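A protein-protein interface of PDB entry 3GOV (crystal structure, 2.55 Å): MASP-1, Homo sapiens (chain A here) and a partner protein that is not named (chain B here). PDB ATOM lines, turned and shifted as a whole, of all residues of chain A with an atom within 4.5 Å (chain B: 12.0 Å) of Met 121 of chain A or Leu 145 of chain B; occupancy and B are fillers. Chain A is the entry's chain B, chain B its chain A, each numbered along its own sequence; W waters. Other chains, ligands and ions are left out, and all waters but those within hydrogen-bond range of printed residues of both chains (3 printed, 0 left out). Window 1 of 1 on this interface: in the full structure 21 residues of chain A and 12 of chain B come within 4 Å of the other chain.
The side-chain hydroxyl (OH) of Tyr 108 of chain B sits at hydrogen-bond distance from the backbone NH (N) of Ala 118 of chain A, at 2.9 Å. The backbone carbonyl oxygen (O) of Cys 143 of chain B sits at hydrogen-bond distance from the side-chain amide nitrogen (NE2) of Gln 211 of chain A (3.2 Å). The backbone carbonyl oxygen (O) of Pro 122 of chain A lies within hydrogen-bond range of the backbone NH (N) of Gly 144 of chain B, 2.8 Å away. SD of Met 121 of chain A sits close to O of Leu 145 of chain B (3.0 Å).
OH of Tyr 109 of chain B lies within hydrogen-bond range of NE2 of His 82 of chain B, at 3.1 Å. The backbone carbonyl oxygen of Tyr 108 of chain B is in hydrogen-bond range of the backbone NH of Val 142 of chain B (3.2 Å). N of Met 121 of chain A lies within hydrogen-bond range of O of Pro 13 of chain A. The backbone NH (N) of Trp 14 of chain A sits close to the backbone carbonyl oxygen (O) of Met 121 of chain A, at 3.4 Å. The backbone carbonyl oxygen of Leu 31 of chain A sits at hydrogen-bond distance from the backbone NH of Ile 123 of chain A (3.0 Å). N of Phe 119 of chain A lies within hydrogen-bond range of OD1 of Asn 117 of chain A, 2.9 Å away.
Among the printed residues, merely in contact across the chains: Trp 14 of chain A with Pro 146 of chain B, Leu 116 of chain A with Tyr 108 of chain B, Leu 116 of chain A with Tyr 109 of chain B, Leu 116 of chain A with Pro 141 of chain B, Asn 117 of chain A with Tyr 108 of chain B, Ala 118 of chain A with Phe 148 of chain B, Phe 119 of chain A with Phe 148 of chain B, Met 121 of chain A with Tyr 108 of chain B, Pro 122 of chain A with Cys 143 of chain B, Ile 123 of chain A with Cys 143 of chain B, Gly 210 of chain A with Gly 144 of chain B, Gly 210 of chain A with Leu 145 of chain B, Gln 211 of chain A with Gly 144 of chain B and Gln 211 of chain A with Leu 145 of chain B.
Printed residues of chain B within 4 Å of Met 121 of chain A: Tyr 108 (3.9 Å) and Leu 145 (3.0 Å). Of chain A, only Met 121, Gly 210 and Gln 211 come within 4 Å of Leu 145 of chain B. No residue of chain B comes within 4 Å of Pro 13 of chain A. Of chain B, only Pro 146 (3.7 Å) comes within 4 Å of Trp 14 of chain A. No residue of chain B comes within 4 Å of Leu 31 of chain A. Leu 116 of chain A touches just these residues of chain B: Tyr 108, Tyr 109 and Pro 141. Asn 117 of chain A touches just one residue of chain B: Tyr 108 (3.3 Å). No residue of chain B comes within 4 Å of Val 120 of chain A. Pro 122 of chain A touches two residues of chain B. Ile 123 of chain A touches just one residue of chain B: Cys 143. Of the printed residues of chain B, Gln 211 of chain A touches Cys 143 (3.2 Å), Gly 144 (3.4 Å) and Leu 145 (3.6 Å). Of the printed residues of chain A, Pro 146 of chain B touches Trp 14. Of the printed residues of chain A, Tyr 108 of chain B touches Leu 116, Asn 117, Ala 118 and Met 121. Printed residues of chain A within 4 Å of Tyr 109 of chain B: Leu 116. Of the printed residues of chain A, Pro 141 of chain B touches Leu 116 (3.7 Å). Of the printed residues of chain A, Cys 143 of chain B touches Pro 122 (3.3 Å), Ile 123 (3.9 Å) and Gln 211 (3.2 Å). Ser 149 of chain B touches none of the printed residues of chain A. The nearest printed residue of chain A that does not touch Leu 145 of chain B is Trp 14 of chain A (4.8 Å). The nearest printed residue of chain A that does not touch Cys 143 of chain B is Met 121 of chain A (5.6 Å).
Hydrophobic or aromatic side chains of chain B within 4 Å of the printed part of chain A: Tyr 108, Tyr 109, Pro 141, Leu 145, Pro 146 and Phe 148. Hydrophobic or aromatic side chains of chain A that line the printed part of chain B: Trp 14, Leu 116, Ala 118, Phe 119 and Met 121. Among the printed residues, 18 pairs touch across the chains. Among the printed residues, no Asp or Glu carboxylate lies within 4 Å of a Lys or Arg side-chain nitrogen of the other chain.
Water W1 lies within hydrogen-bond range of the backbone carbonyl oxygen (O) of Leu 116 of chain A (2.5 Å) and the side-chain amide oxygen (OE1) of Gln 105 of chain B (3.4 Å). Water W2 bridges O of Ala 118 of chain A (2.6 Å) and N of Lys 147 of chain B (2.9 Å). Water W3 lies within hydrogen-bond range of NE2 of Gln 211 of chain A (3.2 Å) and N of Cys 143 of chain B (3.2 Å).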
ATOM      1  N   PRO A  13       9.637  20.844 -13.970  1.00  0.00           N
ATOM      2  CA  PRO A  13       8.558  20.234 -13.185  1.00  0.00           C
ATOM      3  C   PRO A  13       8.959  18.983 -12.387  1.00  0.00           C
ATOM      4  O   PRO A  13       8.184  18.522 -11.565  1.00  0.00           O
ATOM      5  CB  PRO A  13       7.515  19.879 -14.253  1.00  0.00           C
ATOM      6  CG  PRO A  13       8.308  19.663 -15.486  1.00  0.00           C
ATOM      7  CD  PRO A  13       9.444  20.643 -15.416  1.00  0.00           C
ATOM      8  N   TRP A  14      10.162  18.465 -12.622  1.00  0.00           N
ATOM      9  CA  TRP A  14      10.680  17.280 -11.918  1.00  0.00           C
ATOM     10  C   TRP A  14      11.475  17.605 -10.651  1.00  0.00           C
ATOM     11  O   TRP A  14      11.860  16.686  -9.918  1.00  0.00           O
ATOM     12  CB  TRP A  14      11.576  16.458 -12.856  1.00  0.00           C
ATOM     13  CG  TRP A  14      12.466  17.317 -13.664  1.00  0.00           C
ATOM     14  CD1 TRP A  14      13.621  17.911 -13.264  1.00  0.00           C
ATOM     15  CD2 TRP A  14      12.248  17.723 -15.015  1.00  0.00           C
ATOM     16  NE1 TRP A  14      14.148  18.657 -14.293  1.00  0.00           N
ATOM     17  CE2 TRP A  14      13.318  18.558 -15.378  1.00  0.00           C
ATOM     18  CE3 TRP A  14      11.250  17.455 -15.956  1.00  0.00           C
ATOM     19  CZ2 TRP A  14      13.423  19.124 -16.640  1.00  0.00           C
ATOM     20  CZ3 TRP A  14      11.353  18.021 -17.213  1.00  0.00           C
ATOM     21  CH2 TRP A  14      12.430  18.847 -17.544  1.00  0.00           C
ATOM     22  N   LEU A  31      12.035  14.011  -8.982  1.00  0.00           N
ATOM     23  CA  LEU A  31      10.998  12.986  -9.067  1.00  0.00           C
ATOM     24  C   LEU A  31      11.326  11.940 -10.128  1.00  0.00           C
ATOM     25  O   LEU A  31      11.540  12.262 -11.299  1.00  0.00           O
ATOM     26  CB  LEU A  31       9.651  13.624  -9.414  1.00  0.00           C
ATOM     27  CG  LEU A  31       8.429  12.702  -9.487  1.00  0.00           C
ATOM     28  CD1 LEU A  31       8.058  12.191  -8.103  1.00  0.00           C
ATOM     29  CD2 LEU A  31       7.269  13.452 -10.137  1.00  0.00           C
ATOM     30  N   LEU A 116       0.253  14.090 -10.809  1.00  0.00           N
ATOM     31  CA  LEU A 116       1.037  14.506 -11.965  1.00  0.00           C
ATOM     32  C   LEU A 116       0.283  15.540 -12.806  1.00  0.00           C
ATOM     33  O   LEU A 116      -0.933  15.437 -13.000  1.00  0.00           O
ATOM     34  CB  LEU A 116       1.429  13.302 -12.825  1.00  0.00           C
ATOM     35  CG  LEU A 116       2.282  12.209 -12.160  1.00  0.00           C
ATOM     36  CD1 LEU A 116       2.929  11.327 -13.220  1.00  0.00           C
ATOM     37  CD2 LEU A 116       3.347  12.782 -11.225  1.00  0.00           C
ATOM     38  N   ASN A 117       1.018  16.535 -13.294  1.00  0.00           N
ATOM     39  CA  ASN A 117       0.431  17.653 -14.018  1.00  0.00           C
ATOM     40  C   ASN A 117       1.519  18.523 -14.690  1.00  0.00           C
ATOM     41  O   ASN A 117       2.698  18.147 -14.723  1.00  0.00           O
ATOM     42  CB  ASN A 117      -0.420  18.494 -13.061  1.00  0.00           C
ATOM     43  CG  ASN A 117       0.416  19.208 -12.031  1.00  0.00           C
ATOM     44  OD1 ASN A 117       0.754  20.371 -12.199  1.00  0.00           O
ATOM     45  ND2 ASN A 117       0.798  18.499 -10.979  1.00  0.00           N
ATOM     46  N   ALA A 118       1.123  19.686 -15.209  1.00  0.00           N
ATOM     47  CA  ALA A 118       2.036  20.559 -15.948  1.00  0.00           C
ATOM     48  C   ALA A 118       3.220  21.012 -15.106  1.00  0.00           C
ATOM     49  O   ALA A 118       4.284  21.289 -15.644  1.00  0.00           O
ATOM     50  CB  ALA A 118       1.293  21.768 -16.503  1.00  0.00           C
ATOM     51  N   PHE A 119       3.032  21.082 -13.792  1.00  0.00           N
ATOM     52  CA  PHE A 119       4.077  21.543 -12.883  1.00  0.00           C
ATOM     53  C   PHE A 119       4.777  20.427 -12.113  1.00  0.00           C
ATOM     54  O   PHE A 119       5.815  20.663 -11.511  1.00  0.00           O
ATOM     55  CB  PHE A 119       3.497  22.569 -11.911  1.00  0.00           C
ATOM     56  CG  PHE A 119       3.084  23.849 -12.573  1.00  0.00           C
ATOM     57  CD1 PHE A 119       1.759  24.081 -12.904  1.00  0.00           C
ATOM     58  CD2 PHE A 119       4.028  24.817 -12.883  1.00  0.00           C
ATOM     59  CE1 PHE A 119       1.380  25.269 -13.526  1.00  0.00           C
ATOM     60  CE2 PHE A 119       3.662  25.998 -13.507  1.00  0.00           C
ATOM     61  CZ  PHE A 119       2.337  26.224 -13.831  1.00  0.00           C
ATOM     62  N   VAL A 120       4.220  19.220 -12.119  1.00  0.00           N
ATOM     63  CA  VAL A 120       4.845  18.095 -11.422  1.00  0.00           C
ATOM     64  C   VAL A 120       4.805  16.837 -12.284  1.00  0.00           C
ATOM     65  O   VAL A 120       3.771  16.182 -12.398  1.00  0.00           O
ATOM     66  CB  VAL A 120       4.182  17.832 -10.042  1.00  0.00           C
ATOM     67  CG1 VAL A 120       4.876  16.686  -9.323  1.00  0.00           C
ATOM     68  CG2 VAL A 120       4.220  19.087  -9.182  1.00  0.00           C
ATOM     69  N   MET A 121       5.942  16.521 -12.900  1.00  0.00           N
ATOM     70  CA  MET A 121       6.112  15.288 -13.675  1.00  0.00           C
ATOM     71  C   MET A 121       7.557  14.802 -13.516  1.00  0.00           C
ATOM     72  O   MET A 121       8.449  15.604 -13.263  1.00  0.00           O
ATOM     73  CB  MET A 121       5.771  15.529 -15.147  1.00  0.00           C
ATOM     74  CG  MET A 121       6.788  16.361 -15.899  1.00  0.00           C
ATOM     75  SD  MET A 121       6.173  16.906 -17.499  1.00  0.00           S
ATOM     76  CE  MET A 121       5.082  18.256 -17.026  1.00  0.00           C
ATOM     77  N   PRO A 122       7.793  13.487 -13.645  1.00  0.00           N
ATOM     78  CA  PRO A 122       9.131  12.951 -13.410  1.00  0.00           C
ATOM     79  C   PRO A 122      10.133  13.210 -14.525  1.00  0.00           C
ATOM     80  O   PRO A 122       9.751  13.399 -15.684  1.00  0.00           O
ATOM     81  CB  PRO A 122       8.884  11.445 -13.285  1.00  0.00           C
ATOM     82  CG  PRO A 122       7.682  11.195 -14.095  1.00  0.00           C
ATOM     83  CD  PRO A 122       6.825  12.423 -13.966  1.00  0.00           C
ATOM     84  N   ILE A 123      11.412  13.186 -14.151  1.00  0.00           N
ATOM     85  CA  ILE A 123      12.518  13.218 -15.099  1.00  0.00           C
ATOM     86  C   ILE A 123      12.864  11.791 -15.507  1.00  0.00           C
ATOM     87  O   ILE A 123      12.772  10.864 -14.692  1.00  0.00           O
ATOM     88  CB  ILE A 123      13.771  13.887 -14.482  1.00  0.00           C
ATOM     89  CG1 ILE A 123      14.813  14.227 -15.561  1.00  0.00           C
ATOM     90  CG2 ILE A 123      14.383  12.997 -13.399  1.00  0.00           C
ATOM     91  CD1 ILE A 123      14.349  15.255 -16.586  1.00  0.00           C
ATOM     92  N   GLY A 210      12.814  15.068 -27.954  1.00  0.00           N
ATOM     93  CA  GLY A 210      12.346  16.199 -27.164  1.00  0.00           C
ATOM     94  C   GLY A 210      12.173  15.853 -25.692  1.00  0.00           C
ATOM     95  O   GLY A 210      11.453  16.550 -24.975  1.00  0.00           O
ATOM     96  N   GLN A 211      12.835  14.788 -25.232  1.00  0.00           N
ATOM     97  CA  GLN A 211      12.711  14.336 -23.849  1.00  0.00           C
ATOM     98  C   GLN A 211      13.904  14.768 -23.013  1.00  0.00           C
ATOM     99  O   GLN A 211      15.031  14.793 -23.497  1.00  0.00           O
ATOM    100  CB  GLN A 211      12.574  12.815 -23.780  1.00  0.00           C
ATOM    101  CG  GLN A 211      11.157  12.286 -23.914  1.00  0.00           C
ATOM    102  CD  GLN A 211      11.065  10.799 -23.590  1.00  0.00           C
ATOM    103  OE1 GLN A 211      11.872   9.999 -24.069  1.00  0.00           O
ATOM    104  NE2 GLN A 211      10.078  10.425 -22.777  1.00  0.00           N
ATOM    105  N   HIS B  82      -5.524   6.126 -13.023  1.00  0.00           N
ATOM    106  CA  HIS B  82      -4.965   6.969 -14.091  1.00  0.00           C
ATOM    107  C   HIS B  82      -5.437   6.553 -15.485  1.00  0.00           C
ATOM    108  O   HIS B  82      -4.854   6.965 -16.487  1.00  0.00           O
ATOM    109  CB  HIS B  82      -3.433   6.966 -14.054  1.00  0.00           C
ATOM    110  CG  HIS B  82      -2.862   7.149 -12.684  1.00  0.00           C
ATOM    111  ND1 HIS B  82      -2.093   6.187 -12.066  1.00  0.00           N
ATOM    112  CD2 HIS B  82      -2.957   8.175 -11.808  1.00  0.00           C
ATOM    113  CE1 HIS B  82      -1.726   6.620 -10.872  1.00  0.00           C
ATOM    114  NE2 HIS B  82      -2.239   7.823 -10.692  1.00  0.00           N
ATOM    115  N   GLN B 105      -4.638   7.922 -19.075  1.00  0.00           N
ATOM    116  CA  GLN B 105      -4.857   9.373 -19.189  1.00  0.00           C
ATOM    117  C   GLN B 105      -3.658  10.058 -19.840  1.00  0.00           C
ATOM    118  O   GLN B 105      -2.617  10.222 -19.211  1.00  0.00           O
ATOM    119  CB  GLN B 105      -5.102  10.003 -17.803  1.00  0.00           C
ATOM    120  CG  GLN B 105      -5.419  11.522 -17.826  1.00  0.00           C
ATOM    121  CD  GLN B 105      -4.883  12.287 -16.605  1.00  0.00           C
ATOM    122  OE1 GLN B 105      -3.689  12.232 -16.286  1.00  0.00           O
ATOM    123  NE2 GLN B 105      -5.766  13.024 -15.936  1.00  0.00           N
ATOM    124  N   GLU B 106      -3.805  10.465 -21.094  1.00  0.00           N
ATOM    125  CA  GLU B 106      -2.754  11.220 -21.763  1.00  0.00           C
ATOM    126  C   GLU B 106      -2.907  12.656 -21.281  1.00  0.00           C
ATOM    127  O   GLU B 106      -4.022  13.069 -20.967  1.00  0.00           O
ATOM    128  CB  GLU B 106      -2.863  11.095 -23.293  1.00  0.00           C
ATOM    129  CG  GLU B 106      -2.466   9.690 -23.818  1.00  0.00           C
ATOM    130  CD  GLU B 106      -2.539   9.543 -25.350  1.00  0.00           C
ATOM    131  OE1 GLU B 106      -3.646   9.660 -25.929  1.00  0.00           O
ATOM    132  OE2 GLU B 106      -1.491   9.279 -25.978  1.00  0.00           O
ATOM    133  N   PRO B 107      -1.796  13.417 -21.193  1.00  0.00           N
ATOM    134  CA  PRO B 107      -0.420  13.103 -21.581  1.00  0.00           C
ATOM    135  C   PRO B 107       0.478  12.541 -20.471  1.00  0.00           C
ATOM    136  O   PRO B 107       1.557  12.031 -20.775  1.00  0.00           O
ATOM    137  CB  PRO B 107       0.114  14.464 -22.013  1.00  0.00           C
ATOM    138  CG  PRO B 107      -0.595  15.430 -21.107  1.00  0.00           C
ATOM    139  CD  PRO B 107      -1.887  14.786 -20.656  1.00  0.00           C
ATOM    140  N   TYR B 108       0.050  12.622 -19.211  1.00  0.00           N
ATOM    141  CA  TYR B 108       0.925  12.270 -18.073  1.00  0.00           C
ATOM    142  C   TYR B 108       1.018  10.772 -17.752  1.00  0.00           C
ATOM    143  O   TYR B 108       1.702  10.393 -16.799  1.00  0.00           O
ATOM    144  CB  TYR B 108       0.518  13.053 -16.813  1.00  0.00           C
ATOM    145  CG  TYR B 108       0.481  14.541 -17.052  1.00  0.00           C
ATOM    146  CD1 TYR B 108      -0.713  15.242 -17.012  1.00  0.00           C
ATOM    147  CD2 TYR B 108       1.641  15.239 -17.371  1.00  0.00           C
ATOM    148  CE1 TYR B 108      -0.751  16.608 -17.263  1.00  0.00           C
ATOM    149  CE2 TYR B 108       1.618  16.601 -17.620  1.00  0.00           C
ATOM    150  CZ  TYR B 108       0.417  17.281 -17.569  1.00  0.00           C
ATOM    151  OH  TYR B 108       0.387  18.637 -17.820  1.00  0.00           O
ATOM    152  N   TYR B 109       0.346   9.925 -18.533  1.00  0.00           N
ATOM    153  CA  TYR B 109       0.452   8.469 -18.365  1.00  0.00           C
ATOM    154  C   TYR B 109       0.393   7.732 -19.708  1.00  0.00           C
ATOM    155  O   TYR B 109      -0.243   8.195 -20.662  1.00  0.00           O
ATOM    156  CB  TYR B 109      -0.650   7.940 -17.436  1.00  0.00           C
ATOM    157  CG  TYR B 109      -0.548   8.426 -16.010  1.00  0.00           C
ATOM    158  CD1 TYR B 109       0.242   7.763 -15.084  1.00  0.00           C
ATOM    159  CD2 TYR B 109      -1.239   9.551 -15.590  1.00  0.00           C
ATOM    160  CE1 TYR B 109       0.337   8.194 -13.781  1.00  0.00           C
ATOM    161  CE2 TYR B 109      -1.154   9.998 -14.282  1.00  0.00           C
ATOM    162  CZ  TYR B 109      -0.361   9.315 -13.381  1.00  0.00           C
ATOM    163  OH  TYR B 109      -0.262   9.760 -12.086  1.00  0.00           O
ATOM    164  N   LYS B 110       1.086   6.596 -19.774  1.00  0.00           N
ATOM    165  CA  LYS B 110       1.024   5.703 -20.920  1.00  0.00           C
ATOM    166  C   LYS B 110       0.854   4.280 -20.411  1.00  0.00           C
ATOM    167  O   LYS B 110       1.259   3.961 -19.289  1.00  0.00           O
ATOM    168  CB  LYS B 110       2.278   5.824 -21.803  1.00  0.00           C
ATOM    169  CG  LYS B 110       3.592   5.335 -21.172  1.00  0.00           C
ATOM    170  CD  LYS B 110       4.792   5.650 -22.076  1.00  0.00           C
ATOM    171  CE  LYS B 110       6.110   5.116 -21.507  1.00  0.00           C
ATOM    172  NZ  LYS B 110       7.258   5.270 -22.460  1.00  0.00           N
ATOM    173  N   LEU B 140       1.616   3.830 -16.567  1.00  0.00           N
ATOM    174  CA  LEU B 140       2.928   4.279 -16.107  1.00  0.00           C
ATOM    175  C   LEU B 140       3.104   5.755 -16.419  1.00  0.00           C
ATOM    176  O   LEU B 140       2.568   6.233 -17.409  1.00  0.00           O
ATOM    177  CB  LEU B 140       4.043   3.466 -16.767  1.00  0.00           C
ATOM    178  CG  LEU B 140       4.223   2.042 -16.231  1.00  0.00           C
ATOM    179  CD1 LEU B 140       5.220   1.279 -17.079  1.00  0.00           C
ATOM    180  CD2 LEU B 140       4.649   2.040 -14.762  1.00  0.00           C
ATOM    181  N   PRO B 141       3.854   6.482 -15.572  1.00  0.00           N
ATOM    182  CA  PRO B 141       4.037   7.921 -15.761  1.00  0.00           C
ATOM    183  C   PRO B 141       4.925   8.271 -16.952  1.00  0.00           C
ATOM    184  O   PRO B 141       5.988   7.677 -17.108  1.00  0.00           O
ATOM    185  CB  PRO B 141       4.723   8.363 -14.455  1.00  0.00           C
ATOM    186  CG  PRO B 141       4.603   7.214 -13.518  1.00  0.00           C
ATOM    187  CD  PRO B 141       4.568   6.008 -14.376  1.00  0.00           C
ATOM    188  N   VAL B 142       4.502   9.235 -17.774  1.00  0.00           N
ATOM    189  CA  VAL B 142       5.322   9.706 -18.904  1.00  0.00           C
ATOM    190  C   VAL B 142       6.290  10.779 -18.422  1.00  0.00           C
ATOM    191  O   VAL B 142       5.874  11.764 -17.820  1.00  0.00           O
ATOM    192  CB  VAL B 142       4.463  10.262 -20.057  1.00  0.00           C
ATOM    193  CG1 VAL B 142       5.346  10.858 -21.143  1.00  0.00           C
ATOM    194  CG2 VAL B 142       3.580   9.159 -20.630  1.00  0.00           C
ATOM    195  N   CYS B 143       7.580  10.590 -18.696  1.00  0.00           N
ATOM    196  CA  CYS B 143       8.609  11.449 -18.115  1.00  0.00           C
ATOM    197  C   CYS B 143       9.232  12.443 -19.094  1.00  0.00           C
ATOM    198  O   CYS B 143       9.197  12.261 -20.317  1.00  0.00           O
ATOM    199  CB  CYS B 143       9.722  10.603 -17.493  1.00  0.00           C
ATOM    200  SG  CYS B 143      10.617   9.575 -18.668  1.00  0.00           S
ATOM    201  N   GLY B 144       9.792  13.501 -18.514  1.00  0.00           N
ATOM    202  CA  GLY B 144      10.672  14.427 -19.217  1.00  0.00           C
ATOM    203  C   GLY B 144      10.084  15.182 -20.389  1.00  0.00           C
ATOM    204  O   GLY B 144      10.801  15.477 -21.340  1.00  0.00           O
ATOM    205  N   LEU B 145       8.791  15.492 -20.323  1.00  0.00           N
ATOM    206  CA  LEU B 145       8.118  16.264 -21.371  1.00  0.00           C
ATOM    207  C   LEU B 145       7.436  17.483 -20.753  1.00  0.00           C
ATOM    208  O   LEU B 145       6.249  17.426 -20.431  1.00  0.00           O
ATOM    209  CB  LEU B 145       7.095  15.405 -22.125  1.00  0.00           C
ATOM    210  CG  LEU B 145       7.687  14.255 -22.937  1.00  0.00           C
ATOM    211  CD1 LEU B 145       6.583  13.449 -23.564  1.00  0.00           C
ATOM    212  CD2 LEU B 145       8.622  14.772 -23.999  1.00  0.00           C
ATOM    213  N   PRO B 146       8.185  18.598 -20.596  1.00  0.00           N
ATOM    214  CA  PRO B 146       7.630  19.782 -19.956  1.00  0.00           C
ATOM    215  C   PRO B 146       6.650  20.473 -20.864  1.00  0.00           C
ATOM    216  O   PRO B 146       6.743  20.341 -22.090  1.00  0.00           O
ATOM    217  CB  PRO B 146       8.853  20.687 -19.732  1.00  0.00           C
ATOM    218  CG  PRO B 146      10.042  19.899 -20.133  1.00  0.00           C
ATOM    219  CD  PRO B 146       9.574  18.819 -21.030  1.00  0.00           C
ATOM    220  N   LYS B 147       5.732  21.213 -20.255  1.00  0.00           N
ATOM    221  CA  LYS B 147       4.649  21.881 -20.973  1.00  0.00           C
ATOM    222  C   LYS B 147       4.924  23.377 -21.168  1.00  0.00           C
ATOM    223  O   LYS B 147       4.234  24.045 -21.945  1.00  0.00           O
ATOM    224  CB  LYS B 147       3.332  21.662 -20.223  1.00  0.00           C
ATOM    225  CG  LYS B 147       3.023  20.177 -19.929  1.00  0.00           C
ATOM    226  CD  LYS B 147       2.692  19.406 -21.214  1.00  0.00           C
ATOM    227  CE  LYS B 147       2.503  17.902 -20.982  1.00  0.00           C
ATOM    228  NZ  LYS B 147       3.778  17.135 -20.973  1.00  0.00           N
ATOM    229  N   PHE B 148       5.944  23.890 -20.482  1.00  0.00           N
ATOM    230  CA  PHE B 148       6.323  25.298 -20.581  1.00  0.00           C
ATOM    231  C   PHE B 148       7.688  25.419 -21.224  1.00  0.00           C
ATOM    232  O   PHE B 148       8.625  24.732 -20.836  1.00  0.00           O
ATOM    233  CB  PHE B 148       6.326  25.933 -19.196  1.00  0.00           C
ATOM    234  CG  PHE B 148       4.999  25.861 -18.514  1.00  0.00           C
ATOM    235  CD1 PHE B 148       4.748  24.886 -17.564  1.00  0.00           C
ATOM    236  CD2 PHE B 148       3.984  26.744 -18.858  1.00  0.00           C
ATOM    237  CE1 PHE B 148       3.517  24.810 -16.943  1.00  0.00           C
ATOM    238  CE2 PHE B 148       2.750  26.677 -18.247  1.00  0.00           C
ATOM    239  CZ  PHE B 148       2.513  25.706 -17.289  1.00  0.00           C
ATOM    240  N   SER B 149       7.789  26.284 -22.221  1.00  0.00           N
ATOM    241  CA  SER B 149       9.001  26.385 -23.014  1.00  0.00           C
ATOM    242  C   SER B 149      10.055  27.233 -22.308  1.00  0.00           C
ATOM    243  O   SER B 149       9.745  28.038 -21.427  1.00  0.00           O
ATOM    244  CB  SER B 149       8.686  26.985 -24.382  1.00  0.00           C
ATOM    245  OG  SER B 149       8.353  28.353 -24.250  1.00  0.00           O
ATOM    246  N   ARG B 150      11.302  27.053 -22.725  1.00  0.00           N
ATOM    247  CA  ARG B 150      12.419  27.782 -22.148  1.00  0.00           C
ATOM    248  C   ARG B 150      13.148  28.570 -23.224  1.00  0.00           C
ATOM    249  O   ARG B 150      13.466  28.046 -24.288  1.00  0.00           O
ATOM    250  CB  ARG B 150      13.367  26.842 -21.401  1.00  0.00           C
ATOM    251  CG  ARG B 150      13.775  25.588 -22.150  1.00  0.00           C
ATOM    252  CD  ARG B 150      14.471  24.610 -21.217  1.00  0.00           C
ATOM    253  NE  ARG B 150      15.646  25.222 -20.603  1.00  0.00           N
ATOM    254  CZ  ARG B 150      15.859  25.362 -19.297  1.00  0.00           C
ATOM    255  NH1 ARG B 150      15.006  24.901 -18.384  1.00  0.00           N
ATOM    256  NH2 ARG B 150      16.974  25.955 -18.901  1.00  0.00           N
HETATM  257  O   HOH W   1      -2.498  13.469 -13.393  1.00  0.00           O
HETATM  258  O   HOH W   2       6.173  21.574 -17.436  1.00  0.00           O
HETATM  259  O   HOH W   3       7.745   8.756 -21.331  1.00  0.00           O
